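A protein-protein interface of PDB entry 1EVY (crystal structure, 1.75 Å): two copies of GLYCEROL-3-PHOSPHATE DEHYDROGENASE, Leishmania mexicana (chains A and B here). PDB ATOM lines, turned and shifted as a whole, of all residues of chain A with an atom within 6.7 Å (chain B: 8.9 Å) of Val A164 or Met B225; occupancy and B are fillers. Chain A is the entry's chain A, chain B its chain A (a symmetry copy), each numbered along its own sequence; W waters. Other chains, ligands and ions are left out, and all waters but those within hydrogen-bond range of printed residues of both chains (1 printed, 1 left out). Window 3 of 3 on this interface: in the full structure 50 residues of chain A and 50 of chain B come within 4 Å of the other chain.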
ATOM      1  N   LYS A  36     -22.133  -2.510  -0.418  1.00  0.00           N
ATOM      2  CA  LYS A  36     -22.784  -2.093  -1.681  1.00  0.00           C
ATOM      3  C   LYS A  36     -23.948  -2.931  -2.043  1.00  0.00           C
ATOM      4  O   LYS A  36     -24.551  -2.744  -3.092  1.00  0.00           O
ATOM      5  CB  LYS A  36     -21.872  -2.119  -2.932  1.00  0.00           C
ATOM      6  CG  LYS A  36     -20.564  -1.356  -2.765  1.00  0.00           C
ATOM      7  CD  LYS A  36     -19.569  -1.979  -3.744  1.00  0.00           C
ATOM      8  CE  LYS A  36     -18.101  -1.600  -3.590  1.00  0.00           C
ATOM      9  NZ  LYS A  36     -17.341  -2.057  -4.759  1.00  0.00           N
ATOM     10  N   ILE A 158      -6.709  -5.600  -0.276  1.00  0.00           N
ATOM     11  CA  ILE A 158      -6.714  -4.200  -0.676  1.00  0.00           C
ATOM     12  C   ILE A 158      -7.406  -3.977  -1.970  1.00  0.00           C
ATOM     13  O   ILE A 158      -8.180  -3.044  -2.204  1.00  0.00           O
ATOM     14  CB  ILE A 158      -5.316  -3.631  -0.635  1.00  0.00           C
ATOM     15  CG1 ILE A 158      -5.417  -2.191  -1.029  1.00  0.00           C
ATOM     16  CG2 ILE A 158      -4.448  -4.404  -1.618  1.00  0.00           C
ATOM     17  CD1 ILE A 158      -5.630  -1.459   0.285  1.00  0.00           C
ATOM     18  N   GLU A 159      -7.188  -4.923  -2.873  1.00  0.00           N
ATOM     19  CA  GLU A 159      -7.852  -4.687  -4.112  1.00  0.00           C
ATOM     20  C   GLU A 159      -9.338  -4.902  -3.966  1.00  0.00           C
ATOM     21  O   GLU A 159     -10.147  -4.274  -4.647  1.00  0.00           O
ATOM     22  CB  GLU A 159      -7.335  -5.670  -5.255  1.00  0.00           C
ATOM     23  CG  GLU A 159      -5.849  -5.492  -5.696  1.00  0.00           C
ATOM     24  CD  GLU A 159      -5.347  -6.483  -6.778  1.00  0.00           C
ATOM     25  OE1 GLU A 159      -6.062  -7.157  -7.525  1.00  0.00           O
ATOM     26  OE2 GLU A 159      -4.030  -6.489  -6.864  1.00  0.00           O
ATOM     27  N   VAL A 160      -9.715  -5.927  -3.208  1.00  0.00           N
ATOM     28  CA  VAL A 160     -11.170  -6.206  -3.058  1.00  0.00           C
ATOM     29  C   VAL A 160     -11.789  -4.956  -2.356  1.00  0.00           C
ATOM     30  O   VAL A 160     -12.848  -4.502  -2.758  1.00  0.00           O
ATOM     31  CB  VAL A 160     -11.364  -7.475  -2.119  1.00  0.00           C
ATOM     32  CG1 VAL A 160     -12.881  -7.685  -1.789  1.00  0.00           C
ATOM     33  CG2 VAL A 160     -10.746  -8.746  -2.777  1.00  0.00           C
ATOM     34  N   ALA A 161     -11.058  -4.460  -1.320  1.00  0.00           N
ATOM     35  CA  ALA A 161     -11.552  -3.315  -0.558  1.00  0.00           C
ATOM     36  C   ALA A 161     -11.776  -2.056  -1.383  1.00  0.00           C
ATOM     37  O   ALA A 161     -12.794  -1.403  -1.232  1.00  0.00           O
ATOM     38  CB  ALA A 161     -10.668  -3.097   0.632  1.00  0.00           C
ATOM     39  N   THR A 162     -10.883  -1.767  -2.335  1.00  0.00           N
ATOM     40  CA  THR A 162     -10.956  -0.617  -3.225  1.00  0.00           C
ATOM     41  C   THR A 162     -11.744  -0.851  -4.450  1.00  0.00           C
ATOM     42  O   THR A 162     -11.827   0.026  -5.291  1.00  0.00           O
ATOM     43  CB  THR A 162      -9.594  -0.070  -3.519  1.00  0.00           C
ATOM     44  OG1 THR A 162      -8.856  -1.165  -3.919  1.00  0.00           O
ATOM     45  CG2 THR A 162      -9.040   0.284  -2.130  1.00  0.00           C
ATOM     46  N   GLY A 163     -12.406  -1.993  -4.532  1.00  0.00           N
ATOM     47  CA  GLY A 163     -13.287  -2.202  -5.688  1.00  0.00           C
ATOM     48  C   GLY A 163     -12.583  -2.591  -7.000  1.00  0.00           C
ATOM     49  O   GLY A 163     -13.217  -2.480  -8.067  1.00  0.00           O
ATOM     50  N   VAL A 164     -11.295  -2.986  -6.935  1.00  0.00           N
ATOM     51  CA  VAL A 164     -10.555  -3.365  -8.176  1.00  0.00           C
ATOM     52  C   VAL A 164     -11.025  -4.785  -8.566  1.00  0.00           C
ATOM     53  O   VAL A 164     -11.151  -5.622  -7.676  1.00  0.00           O
ATOM     54  CB  VAL A 164      -9.049  -3.319  -7.910  1.00  0.00           C
ATOM     55  CG1 VAL A 164      -8.234  -3.674  -9.168  1.00  0.00           C
ATOM     56  CG2 VAL A 164      -8.716  -1.913  -7.395  1.00  0.00           C
ATOM     57  N   PHE A 165     -11.311  -5.026  -9.852  1.00  0.00           N
ATOM     58  CA  PHE A 165     -11.826  -6.266 -10.447  1.00  0.00           C
ATOM     59  C   PHE A 165     -11.239  -7.518  -9.861  1.00  0.00           C
ATOM     60  O   PHE A 165     -10.021  -7.720  -9.838  1.00  0.00           O
ATOM     61  CB  PHE A 165     -11.748  -6.244 -11.972  1.00  0.00           C
ATOM     62  CG  PHE A 165     -12.482  -7.393 -12.525  1.00  0.00           C
ATOM     63  CD1 PHE A 165     -13.849  -7.313 -12.771  1.00  0.00           C
ATOM     64  CD2 PHE A 165     -11.803  -8.583 -12.796  1.00  0.00           C
ATOM     65  CE1 PHE A 165     -14.553  -8.407 -13.273  1.00  0.00           C
ATOM     66  CE2 PHE A 165     -12.481  -9.663 -13.352  1.00  0.00           C
ATOM     67  CZ  PHE A 165     -13.862  -9.595 -13.535  1.00  0.00           C
ATOM     68  N   THR A 166     -12.173  -8.324  -9.303  1.00  0.00           N
ATOM     69  CA  THR A 166     -11.869  -9.548  -8.573  1.00  0.00           C
ATOM     70  C   THR A 166     -12.895 -10.616  -8.839  1.00  0.00           C
ATOM     71  O   THR A 166     -14.080 -10.318  -8.949  1.00  0.00           O
ATOM     72  CB  THR A 166     -11.772  -9.287  -7.034  1.00  0.00           C
ATOM     73  OG1 THR A 166     -10.690  -8.396  -6.738  1.00  0.00           O
ATOM     74  CG2 THR A 166     -11.468 -10.586  -6.254  1.00  0.00           C
ATOM     75  N   CYS A 167     -12.430 -11.885  -8.964  1.00  0.00           N
ATOM     76  CA  CYS A 167     -13.325 -12.986  -9.198  1.00  0.00           C
ATOM     77  C   CYS A 167     -13.052 -13.968  -8.114  1.00  0.00           C
ATOM     78  O   CYS A 167     -11.918 -14.130  -7.748  1.00  0.00           O
ATOM     79  CB  CYS A 167     -13.041 -13.737 -10.508  1.00  0.00           C
ATOM     80  SG  CYS A 167     -13.594 -12.855 -11.969  1.00  0.00           S
ATOM     81  N   SER A 191     -17.644  -5.530 -10.301  1.00  0.00           N
ATOM     82  CA  SER A 191     -16.259  -5.423  -9.879  1.00  0.00           C
ATOM     83  C   SER A 191     -15.886  -6.601  -8.988  1.00  0.00           C
ATOM     84  O   SER A 191     -14.715  -6.822  -8.687  1.00  0.00           O
ATOM     85  CB  SER A 191     -16.024  -4.127  -9.079  1.00  0.00           C
ATOM     86  OG  SER A 191     -16.864  -4.108  -7.901  1.00  0.00           O
ATOM     87  N   PHE A 192     -16.895  -7.313  -8.442  1.00  0.00           N
ATOM     88  CA  PHE A 192     -16.694  -8.486  -7.536  1.00  0.00           C
ATOM     89  C   PHE A 192     -17.633  -9.486  -8.115  1.00  0.00           C
ATOM     90  O   PHE A 192     -18.824  -9.293  -8.066  1.00  0.00           O
ATOM     91  CB  PHE A 192     -16.971  -8.218  -6.071  1.00  0.00           C
ATOM     92  CG  PHE A 192     -16.475  -9.276  -5.131  1.00  0.00           C
ATOM     93  CD1 PHE A 192     -15.159  -9.283  -4.663  1.00  0.00           C
ATOM     94  CD2 PHE A 192     -17.361 -10.225  -4.619  1.00  0.00           C
ATOM     95  CE1 PHE A 192     -14.685 -10.249  -3.773  1.00  0.00           C
ATOM     96  CE2 PHE A 192     -16.934 -11.213  -3.738  1.00  0.00           C
ATOM     97  CZ  PHE A 192     -15.610 -11.175  -3.293  1.00  0.00           C
ATOM     98  N   GLY B 216      -4.273  -9.847 -23.218  1.00  0.00           N
ATOM     99  CA  GLY B 216      -5.410  -9.567 -22.334  1.00  0.00           C
ATOM    100  C   GLY B 216      -4.859  -9.126 -20.951  1.00  0.00           C
ATOM    101  O   GLY B 216      -5.319  -8.225 -20.279  1.00  0.00           O
ATOM    102  N   SER B 217      -3.807  -9.773 -20.512  1.00  0.00           N
ATOM    103  CA  SER B 217      -3.171  -9.473 -19.242  1.00  0.00           C
ATOM    104  C   SER B 217      -2.627  -8.069 -19.186  1.00  0.00           C
ATOM    105  O   SER B 217      -2.695  -7.368 -18.182  1.00  0.00           O
ATOM    106  CB  SER B 217      -2.088 -10.475 -18.991  1.00  0.00           C
ATOM    107  OG  SER B 217      -1.621 -10.373 -17.678  1.00  0.00           O
ATOM    108  N   GLY B 218      -2.055  -7.631 -20.287  1.00  0.00           N
ATOM    109  CA  GLY B 218      -1.548  -6.276 -20.278  1.00  0.00           C
ATOM    110  C   GLY B 218      -2.716  -5.330 -20.357  1.00  0.00           C
ATOM    111  O   GLY B 218      -2.709  -4.267 -19.736  1.00  0.00           O
ATOM    112  N   VAL B 219      -3.729  -5.754 -21.125  1.00  0.00           N
ATOM    113  CA  VAL B 219      -4.934  -4.950 -21.286  1.00  0.00           C
ATOM    114  C   VAL B 219      -5.446  -4.680 -19.856  1.00  0.00           C
ATOM    115  O   VAL B 219      -5.658  -3.560 -19.436  1.00  0.00           O
ATOM    116  CB  VAL B 219      -6.010  -5.564 -22.238  1.00  0.00           C
ATOM    117  CG1 VAL B 219      -7.394  -4.902 -22.157  1.00  0.00           C
ATOM    118  CG2 VAL B 219      -5.664  -5.330 -23.695  1.00  0.00           C
ATOM    119  N   ALA B 220      -5.628  -5.732 -19.083  1.00  0.00           N
ATOM    120  CA  ALA B 220      -6.095  -5.568 -17.735  1.00  0.00           C
ATOM    121  C   ALA B 220      -5.189  -4.642 -16.956  1.00  0.00           C
ATOM    122  O   ALA B 220      -5.633  -3.841 -16.167  1.00  0.00           O
ATOM    123  CB  ALA B 220      -6.207  -6.916 -17.045  1.00  0.00           C
ATOM    124  N   ASN B 221      -3.906  -4.715 -17.151  1.00  0.00           N
ATOM    125  CA  ASN B 221      -3.028  -3.819 -16.422  1.00  0.00           C
ATOM    126  C   ASN B 221      -3.191  -2.378 -16.878  1.00  0.00           C
ATOM    127  O   ASN B 221      -3.235  -1.430 -16.083  1.00  0.00           O
ATOM    128  CB  ASN B 221      -1.573  -4.200 -16.630  1.00  0.00           C
ATOM    129  CG  ASN B 221      -0.647  -3.213 -15.998  1.00  0.00           C
ATOM    130  OD1 ASN B 221      -0.366  -2.190 -16.616  1.00  0.00           O
ATOM    131  ND2 ASN B 221      -0.180  -3.546 -14.790  1.00  0.00           N
ATOM    132  N   GLY B 222      -3.298  -2.198 -18.171  1.00  0.00           N
ATOM    133  CA  GLY B 222      -3.478  -0.846 -18.653  1.00  0.00           C
ATOM    134  C   GLY B 222      -4.880  -0.266 -18.321  1.00  0.00           C
ATOM    135  O   GLY B 222      -5.129   0.917 -18.407  1.00  0.00           O
ATOM    136  N   LEU B 223      -5.834  -1.075 -17.958  1.00  0.00           N
ATOM    137  CA  LEU B 223      -7.208  -0.630 -17.660  1.00  0.00           C
ATOM    138  C   LEU B 223      -7.358  -0.223 -16.152  1.00  0.00           C
ATOM    139  O   LEU B 223      -8.382   0.294 -15.699  1.00  0.00           O
ATOM    140  CB  LEU B 223      -8.092  -1.865 -17.979  1.00  0.00           C
ATOM    141  CG  LEU B 223      -9.293  -1.733 -18.865  1.00  0.00           C
ATOM    142  CD1 LEU B 223      -9.107  -0.744 -19.997  1.00  0.00           C
ATOM    143  CD2 LEU B 223      -9.661  -3.102 -19.385  1.00  0.00           C
ATOM    144  N   GLY B 224      -6.327  -0.439 -15.346  1.00  0.00           N
ATOM    145  CA  GLY B 224      -6.378  -0.118 -13.918  1.00  0.00           C
ATOM    146  C   GLY B 224      -6.554  -1.325 -12.992  1.00  0.00           C
ATOM    147  O   GLY B 224      -6.454  -1.190 -11.770  1.00  0.00           O
ATOM    148  N   MET B 225      -6.791  -2.520 -13.573  1.00  0.00           N
ATOM    149  CA  MET B 225      -6.981  -3.718 -12.792  1.00  0.00           C
ATOM    150  C   MET B 225      -5.740  -4.184 -12.126  1.00  0.00           C
ATOM    151  O   MET B 225      -4.642  -3.676 -12.397  1.00  0.00           O
ATOM    152  CB  MET B 225      -7.688  -4.757 -13.586  1.00  0.00           C
ATOM    153  CG  MET B 225      -8.846  -4.194 -14.311  1.00  0.00           C
ATOM    154  SD  MET B 225      -9.455  -5.582 -15.266  1.00  0.00           S
ATOM    155  CE  MET B 225     -11.180  -5.175 -15.596  1.00  0.00           C
ATOM    156  N   GLY B 226      -5.869  -5.120 -11.206  1.00  0.00           N
ATOM    157  CA  GLY B 226      -4.683  -5.501 -10.499  1.00  0.00           C
ATOM    158  C   GLY B 226      -4.408  -6.989 -10.640  1.00  0.00           C
ATOM    159  O   GLY B 226      -4.832  -7.600 -11.632  1.00  0.00           O
ATOM    160  N   LEU B 227      -3.689  -7.532  -9.670  1.00  0.00           N
ATOM    161  CA  LEU B 227      -3.309  -8.941  -9.669  1.00  0.00           C
ATOM    162  C   LEU B 227      -4.465  -9.915  -9.515  1.00  0.00           C
ATOM    163  O   LEU B 227      -4.357 -11.064  -9.953  1.00  0.00           O
ATOM    164  CB  LEU B 227      -2.242  -9.192  -8.611  1.00  0.00           C
ATOM    165  CG  LEU B 227      -1.010  -8.322  -8.933  1.00  0.00           C
ATOM    166  CD1 LEU B 227      -0.030  -8.543  -7.808  1.00  0.00           C
ATOM    167  CD2 LEU B 227      -0.369  -8.804 -10.246  1.00  0.00           C
ATOM    168  N   ASN B 228      -5.571  -9.497  -8.859  1.00  0.00           N
ATOM    169  CA  ASN B 228      -6.648 -10.449  -8.723  1.00  0.00           C
ATOM    170  C   ASN B 228      -7.197 -10.665 -10.113  1.00  0.00           C
ATOM    171  O   ASN B 228      -7.570 -11.754 -10.534  1.00  0.00           O
ATOM    172  CB  ASN B 228      -7.805  -9.841  -7.807  1.00  0.00           C
ATOM    173  CG  ASN B 228      -7.422  -9.760  -6.326  1.00  0.00           C
ATOM    174  OD1 ASN B 228      -6.378 -10.253  -5.894  1.00  0.00           O
ATOM    175  ND2 ASN B 228      -8.283  -9.161  -5.512  1.00  0.00           N
ATOM    176  N   ALA B 229      -7.291  -9.574 -10.848  1.00  0.00           N
ATOM    177  CA  ALA B 229      -7.863  -9.697 -12.175  1.00  0.00           C
ATOM    178  C   ALA B 229      -6.997 -10.584 -13.125  1.00  0.00           C
ATOM    179  O   ALA B 229      -7.509 -11.306 -13.991  1.00  0.00           O
ATOM    180  CB  ALA B 229      -7.970  -8.318 -12.743  1.00  0.00           C
ATOM    181  N   ARG B 230      -5.671 -10.492 -12.982  1.00  0.00           N
ATOM    182  CA  ARG B 230      -4.738 -11.279 -13.817  1.00  0.00           C
ATOM    183  C   ARG B 230      -4.918 -12.749 -13.482  1.00  0.00           C
ATOM    184  O   ARG B 230      -4.958 -13.624 -14.355  1.00  0.00           O
ATOM    185  CB  ARG B 230      -3.297 -10.909 -13.489  1.00  0.00           C
ATOM    186  CG  ARG B 230      -2.327 -11.623 -14.454  1.00  0.00           C
ATOM    187  CD  ARG B 230      -0.926 -11.269 -13.983  1.00  0.00           C
ATOM    188  NE  ARG B 230      -0.707  -9.836 -14.309  1.00  0.00           N
ATOM    189  CZ  ARG B 230       0.422  -9.239 -13.880  1.00  0.00           C
ATOM    190  NH1 ARG B 230       1.371  -9.919 -13.208  1.00  0.00           N
ATOM    191  NH2 ARG B 230       0.584  -7.949 -14.143  1.00  0.00           N
ATOM    192  N   ALA B 231      -5.057 -13.014 -12.176  1.00  0.00           N
ATOM    193  CA  ALA B 231      -5.240 -14.396 -11.749  1.00  0.00           C
ATOM    194  C   ALA B 231      -6.528 -14.952 -12.313  1.00  0.00           C
ATOM    195  O   ALA B 231      -6.589 -16.084 -12.753  1.00  0.00           O
ATOM    196  CB  ALA B 231      -5.255 -14.394 -10.275  1.00  0.00           C
ATOM    197  N   ALA B 232      -7.570 -14.130 -12.414  1.00  0.00           N
ATOM    198  CA  ALA B 232      -8.800 -14.641 -12.984  1.00  0.00           C
ATOM    199  C   ALA B 232      -8.692 -14.796 -14.493  1.00  0.00           C
ATOM    200  O   ALA B 232      -9.285 -15.689 -15.066  1.00  0.00           O
ATOM    201  CB  ALA B 232      -9.987 -13.688 -12.676  1.00  0.00           C
ATOM    202  N   LEU B 233      -7.945 -13.899 -15.162  1.00  0.00           N
ATOM    203  CA  LEU B 233      -7.753 -14.014 -16.634  1.00  0.00           C
ATOM    204  C   LEU B 233      -7.012 -15.347 -16.965  1.00  0.00           C
ATOM    205  O   LEU B 233      -7.367 -16.100 -17.847  1.00  0.00           O
ATOM    206  CB  LEU B 233      -6.940 -12.852 -17.196  1.00  0.00           C
ATOM    207  CG  LEU B 233      -6.628 -13.045 -18.684  1.00  0.00           C
ATOM    208  CD1 LEU B 233      -6.676 -11.704 -19.353  1.00  0.00           C
ATOM    209  CD2 LEU B 233      -5.171 -13.423 -18.696  1.00  0.00           C
ATOM    210  N   GLU B 271       5.742  -8.975 -17.242  1.00  0.00           N
ATOM    211  CA  GLU B 271       5.428  -7.551 -17.426  1.00  0.00           C
ATOM    212  C   GLU B 271       6.176  -6.827 -18.487  1.00  0.00           C
ATOM    213  O   GLU B 271       5.698  -5.877 -19.081  1.00  0.00           O
ATOM    214  CB  GLU B 271       5.370  -6.719 -16.127  1.00  0.00           C
ATOM    215  CG  GLU B 271       4.250  -7.208 -15.194  1.00  0.00           C
ATOM    216  CD  GLU B 271       3.949  -6.343 -13.979  1.00  0.00           C
ATOM    217  OE1 GLU B 271       4.749  -5.579 -13.471  1.00  0.00           O
ATOM    218  OE2 GLU B 271       2.727  -6.525 -13.503  1.00  0.00           O
ATOM    219  N   PHE B 276       2.507  -8.258 -23.324  1.00  0.00           N
ATOM    220  CA  PHE B 276       2.056  -7.491 -22.144  1.00  0.00           C
ATOM    221  C   PHE B 276       2.098  -5.981 -22.418  1.00  0.00           C
ATOM    222  O   PHE B 276       1.111  -5.232 -22.250  1.00  0.00           O
ATOM    223  CB  PHE B 276       2.918  -7.887 -20.923  1.00  0.00           C
ATOM    224  CG  PHE B 276       2.290  -7.396 -19.630  1.00  0.00           C
ATOM    225  CD1 PHE B 276       1.546  -8.262 -18.817  1.00  0.00           C
ATOM    226  CD2 PHE B 276       2.430  -6.061 -19.233  1.00  0.00           C
ATOM    227  CE1 PHE B 276       0.944  -7.840 -17.631  1.00  0.00           C
ATOM    228  CE2 PHE B 276       1.842  -5.599 -18.048  1.00  0.00           C
ATOM    229  CZ  PHE B 276       1.093  -6.495 -17.278  1.00  0.00           C
ATOM    230  N   GLY B 283      -4.856  -1.045 -23.544  1.00  0.00           N
ATOM    231  CA  GLY B 283      -5.611  -0.896 -22.335  1.00  0.00           C
ATOM    232  C   GLY B 283      -5.585   0.570 -21.921  1.00  0.00           C
ATOM    233  O   GLY B 283      -6.593   1.104 -21.440  1.00  0.00           O
ATOM    234  N   PRO B 335     -11.596  -1.330 -25.164  1.00  0.00           N
ATOM    235  CA  PRO B 335     -11.335  -2.315 -24.142  1.00  0.00           C
ATOM    236  C   PRO B 335     -12.342  -2.381 -23.037  1.00  0.00           C
ATOM    237  O   PRO B 335     -12.667  -3.471 -22.545  1.00  0.00           O
ATOM    238  CB  PRO B 335      -9.920  -2.083 -23.638  1.00  0.00           C
ATOM    239  CG  PRO B 335      -9.329  -1.020 -24.536  1.00  0.00           C
ATOM    240  CD  PRO B 335     -10.375  -0.618 -25.573  1.00  0.00           C
ATOM    241  N   ARG B 336     -12.822  -1.204 -22.643  1.00  0.00           N
ATOM    242  CA  ARG B 336     -13.795  -1.112 -21.578  1.00  0.00           C
ATOM    243  C   ARG B 336     -15.112  -1.715 -22.042  1.00  0.00           C
ATOM    244  O   ARG B 336     -15.851  -2.384 -21.312  1.00  0.00           O
ATOM    245  CB  ARG B 336     -13.881   0.323 -21.055  1.00  0.00           C
ATOM    246  CG  ARG B 336     -13.835   0.394 -19.551  1.00  0.00           C
ATOM    247  CD  ARG B 336     -13.196   1.677 -19.093  1.00  0.00           C
ATOM    248  NE  ARG B 336     -12.334   1.375 -17.999  1.00  0.00           N
ATOM    249  CZ  ARG B 336     -11.195   2.019 -17.835  1.00  0.00           C
ATOM    250  NH1 ARG B 336     -10.799   3.026 -18.655  1.00  0.00           N
ATOM    251  NH2 ARG B 336     -10.476   1.621 -16.786  1.00  0.00           N
ATOM    252  N   ALA B 338     -15.207  -4.025 -24.372  1.00  0.00           N
ATOM    253  CA  ALA B 338     -14.946  -5.454 -24.483  1.00  0.00           C
ATOM    254  C   ALA B 338     -15.133  -6.092 -23.114  1.00  0.00           C
ATOM    255  O   ALA B 338     -15.769  -7.145 -23.007  1.00  0.00           O
ATOM    256  CB  ALA B 338     -13.531  -5.660 -24.982  1.00  0.00           C
ATOM    257  N   LEU B 339     -14.597  -5.424 -22.044  1.00  0.00           N
ATOM    258  CA  LEU B 339     -14.713  -5.982 -20.686  1.00  0.00           C
ATOM    259  C   LEU B 339     -16.167  -6.137 -20.278  1.00  0.00           C
ATOM    260  O   LEU B 339     -16.643  -7.122 -19.664  1.00  0.00           O
ATOM    261  CB  LEU B 339     -14.003  -5.017 -19.760  1.00  0.00           C
ATOM    262  CG  LEU B 339     -13.463  -5.571 -18.453  1.00  0.00           C
ATOM    263  CD1 LEU B 339     -13.563  -4.504 -17.358  1.00  0.00           C
ATOM    264  CD2 LEU B 339     -14.031  -6.942 -18.118  1.00  0.00           C
ATOM    265  N   ALA B 340     -16.912  -5.115 -20.677  1.00  0.00           N
ATOM    266  CA  ALA B 340     -18.314  -5.125 -20.345  1.00  0.00           C
ATOM    267  C   ALA B 340     -19.060  -6.216 -21.055  1.00  0.00           C
ATOM    268  O   ALA B 340     -19.908  -6.869 -20.439  1.00  0.00           O
ATOM    269  CB  ALA B 340     -18.923  -3.796 -20.710  1.00  0.00           C
ATOM    270  N   LEU B 342     -17.756  -8.848 -22.174  1.00  0.00           N
ATOM    271  CA  LEU B 342     -17.268 -10.051 -21.570  1.00  0.00           C
ATOM    272  C   LEU B 342     -18.046 -10.262 -20.298  1.00  0.00           C
ATOM    273  O   LEU B 342     -18.433 -11.374 -19.988  1.00  0.00           O
ATOM    274  CB  LEU B 342     -15.840  -9.770 -21.127  1.00  0.00           C
ATOM    275  CG  LEU B 342     -14.765 -10.792 -21.457  1.00  0.00           C
ATOM    276  CD1 LEU B 342     -13.889 -10.965 -20.239  1.00  0.00           C
ATOM    277  CD2 LEU B 342     -15.297 -12.153 -21.893  1.00  0.00           C
ATOM    278  N   LEU B 343     -18.255  -9.188 -19.527  1.00  0.00           N
ATOM    279  CA  LEU B 343     -18.964  -9.398 -18.276  1.00  0.00           C
ATOM    280  C   LEU B 343     -20.441  -9.560 -18.415  1.00  0.00           C
ATOM    281  O   LEU B 343     -21.115  -9.770 -17.436  1.00  0.00           O
ATOM    282  CB  LEU B 343     -18.634  -8.415 -17.148  1.00  0.00           C
ATOM    283  CG  LEU B 343     -17.137  -8.408 -16.856  1.00  0.00           C
ATOM    284  CD1 LEU B 343     -16.767  -7.201 -16.043  1.00  0.00           C
ATOM    285  CD2 LEU B 343     -16.772  -9.646 -16.079  1.00  0.00           C
HETATM  286  O   HOH W   1      -9.736 -12.607  -8.925  1.00  0.00           O
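Water W1 bridges the backbone NH (N) of Cys A167 (2.8 Å) and the backbone carbonyl oxygen (O) of Asn B228 (2.8 Å).
No position is printed for both chains.
The backbone NH of Leu B227 sits at hydrogen-bond distance from the side-chain carboxylate of Glu A159.
The side-chain carboxylate of Glu A159 is in hydrogen-bond range of the backbone NH of Asn B228.
The backbone carbonyl oxygen (O) of Phe A165 sits at hydrogen-bond distance from the backbone NH (N) of Ala B229.
The side-chain hydroxyl (OG1) of Thr A166 lies within hydrogen-bond range of the side-chain amide nitrogen (ND2) of Asn B228.
Of the 13 printed residues of chain A, 6 touch a printed residue of chain B.
Among the printed residues, 12 pairs touch across the chains.
Among the printed residues, no Asp or Glu carboxylate lies within 4 Å of a Lys or Arg side-chain nitrogen of the other chain.
The backbone carbonyl oxygen of Glu A159 is in hydrogen-bond range of the side-chain hydroxyl of Thr A162.
N of Val A164 is in hydrogen-bond range of O of Glu A159 (2.9 Å).
OG1 of Thr A166 lies within hydrogen-bond range of O of Val A164 (3.0 Å).
N of Thr A166 is in hydrogen-bond range of O of Ser A191, 3.0 Å away.
N of Met B225 is in hydrogen-bond range of O of Ala B220, at 3.1 Å.
Of the printed residues of chain B, Val A164 touches Met B225 and Gly B226.
Met B225 touches just these residues of chain A: Val A164 (3.8 Å) and Phe A165 (3.8 Å).
No residue of chain B comes within 4 Å of Gly A163.
Of the printed residues of chain A, Leu B343 touches Phe A165 (3.7 Å).
Of the printed residues of chain A, Ala B232 touches Cys A167.
Of the printed residues of chain A, Gly B226 touches Glu A159 (3.5 Å) and Val A164 (3.4 Å).
Phe B276 touches none of the printed residues of chain A.
The nearest printed residue of chain B that does not touch Val A164 is Gly B224 (4.01 Å).
Glu A159 touches Gly B226.
Asn B228 touches Val A160 (ND2 to CG2, 3.7 Å).
Met B225 touches Val A164 (CA to CG1, 3.8 Å).
Val A164 touches Gly B226 (CG1 to N, 3.4 Å).
Met B225 touches Phe A165 (CE to CB, 3.8 Å).
Phe A165 touches Asn B228 (O to CB, 3.7 Å).
Leu B343 touches Phe A165.
CB of Cys A167 touches CB of Ala B232, 3.7 Å away.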
